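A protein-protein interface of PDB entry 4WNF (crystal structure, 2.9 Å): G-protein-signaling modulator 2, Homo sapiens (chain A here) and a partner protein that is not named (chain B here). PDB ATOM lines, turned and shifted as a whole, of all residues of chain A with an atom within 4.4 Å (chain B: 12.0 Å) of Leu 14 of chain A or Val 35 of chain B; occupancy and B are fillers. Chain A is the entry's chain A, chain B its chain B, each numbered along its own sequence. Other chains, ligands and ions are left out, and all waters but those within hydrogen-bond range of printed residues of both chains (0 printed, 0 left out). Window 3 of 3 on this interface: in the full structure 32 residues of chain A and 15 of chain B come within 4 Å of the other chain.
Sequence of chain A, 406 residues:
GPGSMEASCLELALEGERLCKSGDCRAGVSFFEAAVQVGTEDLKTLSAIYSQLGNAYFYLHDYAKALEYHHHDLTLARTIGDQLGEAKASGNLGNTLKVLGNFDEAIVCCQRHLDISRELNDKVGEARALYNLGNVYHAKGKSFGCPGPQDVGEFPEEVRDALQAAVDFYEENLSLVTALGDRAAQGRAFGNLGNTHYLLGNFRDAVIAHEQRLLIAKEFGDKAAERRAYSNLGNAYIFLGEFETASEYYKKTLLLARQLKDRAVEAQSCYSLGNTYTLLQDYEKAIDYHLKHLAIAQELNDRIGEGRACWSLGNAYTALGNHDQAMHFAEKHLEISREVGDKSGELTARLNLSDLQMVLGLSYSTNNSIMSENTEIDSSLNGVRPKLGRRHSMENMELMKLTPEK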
ATOM      1  N   LEU A  10     -20.943 -27.359  22.157  1.00  0.00           N
ATOM      2  CA  LEU A  10     -21.311 -26.730  20.907  1.00  0.00           C
ATOM      3  C   LEU A  10     -20.335 -27.179  19.827  1.00  0.00           C
ATOM      4  O   LEU A  10     -20.746 -27.518  18.719  1.00  0.00           O
ATOM      5  CB  LEU A  10     -21.342 -25.200  21.047  1.00  0.00           C
ATOM      6  CG  LEU A  10     -22.274 -24.407  20.108  1.00  0.00           C
ATOM      7  CD1 LEU A  10     -23.704 -24.945  20.093  1.00  0.00           C
ATOM      8  CD2 LEU A  10     -22.276 -22.923  20.480  1.00  0.00           C
ATOM      9  N   GLU A  11     -19.048 -27.213  20.165  1.00  0.00           N
ATOM     10  CA  GLU A  11     -18.016 -27.635  19.213  1.00  0.00           C
ATOM     11  C   GLU A  11     -18.271 -29.042  18.698  1.00  0.00           C
ATOM     12  O   GLU A  11     -18.245 -29.292  17.503  1.00  0.00           O
ATOM     13  CB  GLU A  11     -16.624 -27.612  19.853  1.00  0.00           C
ATOM     14  CG  GLU A  11     -16.011 -26.235  20.037  1.00  0.00           C
ATOM     15  CD  GLU A  11     -14.931 -26.223  21.110  1.00  0.00           C
ATOM     16  OE1 GLU A  11     -14.414 -27.314  21.476  1.00  0.00           O
ATOM     17  OE2 GLU A  11     -14.615 -25.114  21.601  1.00  0.00           O
ATOM     18  N   LEU A  12     -18.502 -29.965  19.612  1.00  0.00           N
ATOM     19  CA  LEU A  12     -18.576 -31.361  19.240  1.00  0.00           C
ATOM     20  C   LEU A  12     -19.746 -31.656  18.310  1.00  0.00           C
ATOM     21  O   LEU A  12     -19.647 -32.508  17.416  1.00  0.00           O
ATOM     22  CB  LEU A  12     -18.647 -32.214  20.494  1.00  0.00           C
ATOM     23  CG  LEU A  12     -17.302 -32.210  21.226  1.00  0.00           C
ATOM     24  CD1 LEU A  12     -17.450 -32.422  22.726  1.00  0.00           C
ATOM     25  CD2 LEU A  12     -16.393 -33.270  20.619  1.00  0.00           C
ATOM     26  N   ALA A  13     -20.842 -30.932  18.515  1.00  0.00           N
ATOM     27  CA  ALA A  13     -22.035 -31.081  17.688  1.00  0.00           C
ATOM     28  C   ALA A  13     -21.804 -30.540  16.299  1.00  0.00           C
ATOM     29  O   ALA A  13     -22.045 -31.236  15.309  1.00  0.00           O
ATOM     30  CB  ALA A  13     -23.197 -30.355  18.325  1.00  0.00           C
ATOM     31  N   LEU A  14     -21.348 -29.290  16.236  1.00  0.00           N
ATOM     32  CA  LEU A  14     -20.922 -28.666  14.982  1.00  0.00           C
ATOM     33  C   LEU A  14     -20.055 -29.596  14.152  1.00  0.00           C
ATOM     34  O   LEU A  14     -20.313 -29.807  12.965  1.00  0.00           O
ATOM     35  CB  LEU A  14     -20.147 -27.383  15.261  1.00  0.00           C
ATOM     36  CG  LEU A  14     -21.003 -26.176  15.660  1.00  0.00           C
ATOM     37  CD1 LEU A  14     -20.126 -25.054  16.203  1.00  0.00           C
ATOM     38  CD2 LEU A  14     -21.843 -25.673  14.489  1.00  0.00           C
ATOM     39  N   GLU A  15     -19.031 -30.157  14.782  1.00  0.00           N
ATOM     40  CA  GLU A  15     -18.230 -31.157  14.117  1.00  0.00           C
ATOM     41  C   GLU A  15     -19.161 -32.216  13.562  1.00  0.00           C
ATOM     42  O   GLU A  15     -19.284 -32.362  12.351  1.00  0.00           O
ATOM     43  CB  GLU A  15     -17.209 -31.774  15.074  1.00  0.00           C
ATOM     44  CG  GLU A  15     -16.227 -32.726  14.399  1.00  0.00           C
ATOM     45  CD  GLU A  15     -15.268 -32.041  13.428  1.00  0.00           C
ATOM     46  OE1 GLU A  15     -15.322 -30.790  13.273  1.00  0.00           O
ATOM     47  OE2 GLU A  15     -14.451 -32.771  12.819  1.00  0.00           O
ATOM     48  N   GLY A  16     -19.867 -32.905  14.451  1.00  0.00           N
ATOM     49  CA  GLY A  16     -20.759 -33.992  14.059  1.00  0.00           C
ATOM     50  C   GLY A  16     -21.612 -33.693  12.840  1.00  0.00           C
ATOM     51  O   GLY A  16     -21.873 -34.585  12.012  1.00  0.00           O
ATOM     52  N   GLU A  17     -22.056 -32.440  12.731  1.00  0.00           N
ATOM     53  CA  GLU A  17     -22.894 -32.025  11.612  1.00  0.00           C
ATOM     54  C   GLU A  17     -22.119 -32.094  10.311  1.00  0.00           C
ATOM     55  O   GLU A  17     -22.589 -32.705   9.352  1.00  0.00           O
ATOM     56  CB  GLU A  17     -23.452 -30.621  11.827  1.00  0.00           C
ATOM     57  CG  GLU A  17     -24.489 -30.534  12.935  1.00  0.00           C
ATOM     58  CD  GLU A  17     -25.469 -29.387  12.742  1.00  0.00           C
ATOM     59  OE1 GLU A  17     -26.043 -28.922  13.744  1.00  0.00           O
ATOM     60  OE2 GLU A  17     -25.700 -28.966  11.588  1.00  0.00           O
ATOM     61  N   ARG A  18     -20.927 -31.498  10.287  1.00  0.00           N
ATOM     62  CA  ARG A  18     -20.098 -31.534   9.082  1.00  0.00           C
ATOM     63  C   ARG A  18     -19.747 -32.983   8.711  1.00  0.00           C
ATOM     64  O   ARG A  18     -19.674 -33.334   7.531  1.00  0.00           O
ATOM     65  CB  ARG A  18     -18.848 -30.634   9.215  1.00  0.00           C
ATOM     66  CG  ARG A  18     -17.605 -31.245   9.853  1.00  0.00           C
ATOM     67  CD  ARG A  18     -16.383 -30.329   9.713  1.00  0.00           C
ATOM     68  NE  ARG A  18     -15.139 -31.008  10.088  1.00  0.00           N
ATOM     69  CZ  ARG A  18     -14.521 -31.936   9.351  1.00  0.00           C
ATOM     70  NH1 ARG A  18     -15.014 -32.317   8.173  1.00  0.00           N
ATOM     71  NH2 ARG A  18     -13.395 -32.493   9.789  1.00  0.00           N
ATOM     72  N   THR A  45     -30.348 -26.504  21.873  1.00  0.00           N
ATOM     73  CA  THR A  45     -29.185 -27.195  21.351  1.00  0.00           C
ATOM     74  C   THR A  45     -29.248 -28.695  21.591  1.00  0.00           C
ATOM     75  O   THR A  45     -29.016 -29.484  20.674  1.00  0.00           O
ATOM     76  CB  THR A  45     -27.889 -26.683  21.999  1.00  0.00           C
ATOM     77  OG1 THR A  45     -27.824 -25.248  21.925  1.00  0.00           O
ATOM     78  CG2 THR A  45     -26.694 -27.276  21.293  1.00  0.00           C
ATOM     79  N   ALA A  48     -31.745 -30.328  19.339  1.00  0.00           N
ATOM     80  CA  ALA A  48     -31.159 -30.468  18.032  1.00  0.00           C
ATOM     81  C   ALA A  48     -30.297 -31.733  17.969  1.00  0.00           C
ATOM     82  O   ALA A  48     -30.420 -32.541  17.050  1.00  0.00           O
ATOM     83  CB  ALA A  48     -30.342 -29.236  17.699  1.00  0.00           C
ATOM     84  N   ILE A  49     -29.465 -31.925  18.982  1.00  0.00           N
ATOM     85  CA  ILE A  49     -28.473 -32.989  18.946  1.00  0.00           C
ATOM     86  C   ILE A  49     -29.122 -34.360  18.956  1.00  0.00           C
ATOM     87  O   ILE A  49     -28.723 -35.243  18.209  1.00  0.00           O
ATOM     88  CB  ILE A  49     -27.481 -32.866  20.116  1.00  0.00           C
ATOM     89  CG1 ILE A  49     -26.704 -31.550  19.993  1.00  0.00           C
ATOM     90  CG2 ILE A  49     -26.511 -34.045  20.128  1.00  0.00           C
ATOM     91  CD1 ILE A  49     -26.211 -30.995  21.309  1.00  0.00           C
ATOM     92  N   GLU B  31     -37.160 -34.843   8.701  1.00  0.00           N
ATOM     93  CA  GLU B  31     -36.895 -33.431   8.979  1.00  0.00           C
ATOM     94  C   GLU B  31     -35.637 -33.368   9.828  1.00  0.00           C
ATOM     95  O   GLU B  31     -35.320 -34.337  10.516  1.00  0.00           O
ATOM     96  CB  GLU B  31     -38.050 -32.752   9.710  1.00  0.00           C
ATOM     97  CG  GLU B  31     -39.444 -33.170   9.268  1.00  0.00           C
ATOM     98  CD  GLU B  31     -39.599 -33.264   7.764  1.00  0.00           C
ATOM     99  OE1 GLU B  31     -39.924 -34.390   7.248  1.00  0.00           O
ATOM    100  OE2 GLU B  31     -39.385 -32.208   7.114  1.00  0.00           O
ATOM    101  N   THR B  32     -34.918 -32.245   9.765  1.00  0.00           N
ATOM    102  CA  THR B  32     -33.569 -32.157  10.335  1.00  0.00           C
ATOM    103  C   THR B  32     -33.316 -30.861  11.113  1.00  0.00           C
ATOM    104  O   THR B  32     -33.512 -29.775  10.615  1.00  0.00           O
ATOM    105  CB  THR B  32     -32.477 -32.269   9.237  1.00  0.00           C
ATOM    106  OG1 THR B  32     -32.525 -31.116   8.406  1.00  0.00           O
ATOM    107  CG2 THR B  32     -32.658 -33.513   8.363  1.00  0.00           C
ATOM    108  N   LYS B  33     -32.823 -30.991  12.327  1.00  0.00           N
ATOM    109  CA  LYS B  33     -32.541 -29.840  13.143  1.00  0.00           C
ATOM    110  C   LYS B  33     -31.042 -29.610  13.208  1.00  0.00           C
ATOM    111  O   LYS B  33     -30.261 -30.561  13.208  1.00  0.00           O
ATOM    112  CB  LYS B  33     -33.075 -30.067  14.564  1.00  0.00           C
ATOM    113  CG  LYS B  33     -34.520 -30.548  14.655  1.00  0.00           C
ATOM    114  CD  LYS B  33     -35.088 -30.195  16.011  1.00  0.00           C
ATOM    115  CE  LYS B  33     -36.437 -30.824  16.269  1.00  0.00           C
ATOM    116  NZ  LYS B  33     -36.847 -30.504  17.666  1.00  0.00           N
ATOM    117  N   SER B  34     -30.645 -28.350  13.318  1.00  0.00           N
ATOM    118  CA  SER B  34     -29.243 -28.002  13.437  1.00  0.00           C
ATOM    119  C   SER B  34     -28.946 -27.198  14.703  1.00  0.00           C
ATOM    120  O   SER B  34     -29.780 -26.426  15.179  1.00  0.00           O
ATOM    121  CB  SER B  34     -28.817 -27.200  12.219  1.00  0.00           C
ATOM    122  OG  SER B  34     -27.523 -26.686  12.408  1.00  0.00           O
ATOM    123  N   VAL B  35     -27.748 -27.401  15.243  1.00  0.00           N
ATOM    124  CA  VAL B  35     -27.170 -26.498  16.244  1.00  0.00           C
ATOM    125  C   VAL B  35     -27.007 -25.085  15.693  1.00  0.00           C
ATOM    126  O   VAL B  35     -27.143 -24.114  16.428  1.00  0.00           O
ATOM    127  CB  VAL B  35     -25.778 -26.977  16.721  1.00  0.00           C
ATOM    128  CG1 VAL B  35     -25.907 -28.242  17.534  1.00  0.00           C
ATOM    129  CG2 VAL B  35     -24.831 -27.236  15.556  1.00  0.00           C
ATOM    130  N   THR B  36     -26.723 -24.995  14.389  1.00  0.00           N
ATOM    131  CA  THR B  36     -26.426 -23.731  13.697  1.00  0.00           C
ATOM    132  C   THR B  36     -27.651 -22.823  13.684  1.00  0.00           C
ATOM    133  O   THR B  36     -27.554 -21.645  13.336  1.00  0.00           O
ATOM    134  CB  THR B  36     -25.994 -23.929  12.205  1.00  0.00           C
ATOM    135  OG1 THR B  36     -27.151 -24.093  11.367  1.00  0.00           O
ATOM    136  CG2 THR B  36     -25.014 -25.127  11.999  1.00  0.00           C
ATOM    137  N   ASP B  37     -28.808 -23.392  14.019  1.00  0.00           N
ATOM    138  CA  ASP B  37     -30.046 -22.629  14.155  1.00  0.00           C
ATOM    139  C   ASP B  37     -29.928 -21.519  15.209  1.00  0.00           C
ATOM    140  O   ASP B  37     -30.593 -20.483  15.097  1.00  0.00           O
ATOM    141  CB  ASP B  37     -31.213 -23.564  14.499  1.00  0.00           C
ATOM    142  CG  ASP B  37     -31.568 -24.519  13.352  1.00  0.00           C
ATOM    143  OD1 ASP B  37     -31.346 -24.160  12.172  1.00  0.00           O
ATOM    144  OD2 ASP B  37     -32.081 -25.627  13.637  1.00  0.00           O
ATOM    145  N   TYR B  38     -29.097 -21.747  16.233  1.00  0.00           N
ATOM    146  CA  TYR B  38     -28.685 -20.683  17.157  1.00  0.00           C
ATOM    147  C   TYR B  38     -28.280 -19.443  16.339  1.00  0.00           C
ATOM    148  O   TYR B  38     -28.811 -18.350  16.544  1.00  0.00           O
ATOM    149  CB  TYR B  38     -27.510 -21.151  18.047  1.00  0.00           C
ATOM    150  CG  TYR B  38     -27.449 -20.549  19.451  1.00  0.00           C
ATOM    151  CD1 TYR B  38     -28.109 -19.353  19.772  1.00  0.00           C
ATOM    152  CD2 TYR B  38     -26.695 -21.165  20.455  1.00  0.00           C
ATOM    153  CE1 TYR B  38     -28.040 -18.810  21.049  1.00  0.00           C
ATOM    154  CE2 TYR B  38     -26.617 -20.624  21.733  1.00  0.00           C
ATOM    155  CZ  TYR B  38     -27.292 -19.447  22.028  1.00  0.00           C
ATOM    156  OH  TYR B  38     -27.227 -18.898  23.294  1.00  0.00           O
ATOM    157  N   PHE B  39     -27.362 -19.640  15.390  1.00  0.00           N
ATOM    158  CA  PHE B  39     -26.903 -18.570  14.494  1.00  0.00           C
ATOM    159  C   PHE B  39     -27.851 -18.390  13.298  1.00  0.00           C
ATOM    160  O   PHE B  39     -28.768 -17.563  13.321  1.00  0.00           O
ATOM    161  CB  PHE B  39     -25.486 -18.875  13.991  1.00  0.00           C
ATOM    162  CG  PHE B  39     -24.634 -17.652  13.802  1.00  0.00           C
ATOM    163  CD1 PHE B  39     -24.606 -16.981  12.580  1.00  0.00           C
ATOM    164  CD2 PHE B  39     -23.857 -17.164  14.851  1.00  0.00           C
ATOM    165  CE1 PHE B  39     -23.816 -15.846  12.412  1.00  0.00           C
ATOM    166  CE2 PHE B  39     -23.067 -16.032  14.686  1.00  0.00           C
ATOM    167  CZ  PHE B  39     -23.047 -15.371  13.464  1.00  0.00           C
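The side-chain hydroxyl (OG) of Ser 34 of chain B lies within hydrogen-bond range of the side-chain carboxylate (OE1) of Glu 17 of chain A, at 3.0 Å. OE1 of Glu 17 of chain A sits at hydrogen-bond distance from N of Val 35 of chain B (2.7 Å).
The side-chain hydroxyl of Ser 34 of chain B lies within hydrogen-bond range of the backbone NH of Thr 36 of chain B (2.7 Å). The backbone NH (N) of Ser 34 of chain B sits at hydrogen-bond distance from the side-chain carboxylate (OD2) of Asp 37 of chain B (3.1 Å).
CG1 of Val 35 of chain B touches CB of Ala 13 of chain A, 3.5 Å away. Val 35 of chain B touches Leu 14 of chain A (CG2 to CD2, 3.5 Å). Glu 17 of chain A touches Thr 36 of chain B (OE2 to CG2, 3.9 Å). Thr 45 of chain A touches Val 35 of chain B (CG2 to CG1, 3.96 Å). CA of Ala 48 of chain A touches CB of Lys 33 of chain B, at 3.98 Å. Ala 48 of chain A touches Ser 34 of chain B.
Leu 14 of chain A touches just one residue of chain B: Val 35 (3.5 Å). No residue of chain B comes within 4 Å of Leu 10 of chain A. Ala 13 of chain A touches just one residue of chain B: Val 35 (3.5 Å). No residue of chain B comes within 4 Å of Gly 16 of chain A. Of chain B, only Ser 34, Val 35 and Thr 36 come within 4 Å of Glu 17 of chain A. Thr 45 of chain A touches just one residue of chain B: Val 35. Printed residues of chain B within 4 Å of Ala 48 of chain A: Lys 33 and Ser 34. Printed residues of chain A within 4 Å of Lys 33 of chain B: Ala 48 (3.98 Å). Of the printed residues of chain A, Ser 34 of chain B touches Glu 17 and Ala 48. Of the printed residues of chain A, Thr 36 of chain B touches Glu 17 (3.9 Å). Phe 39 of chain B touches none of the printed residues of chain A. Asp 37 of chain B touches none of the printed residues of chain A. The nearest printed residue of chain A that does not touch Val 35 of chain B is Ala 48 of chain A (4.02 Å). The nearest printed residue of chain B that does not touch Ala 48 of chain A is Val 35 of chain B (4.02 Å).
Printed residues of chain B that touch a printed residue of chain A: Lys 33, Ser 34, Val 35 and Thr 36. Of the 12 printed residues of chain A, 5 touch a printed residue of chain B. Printed residues of chain A that touch a printed residue of chain B: Ala 13, Leu 14, Glu 17, Thr 45 and Ala 48. Among the printed residues, no Asp or Glu carboxylate lies within 4 Å of a Lys or Arg side-chain nitrogen of the other chain.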
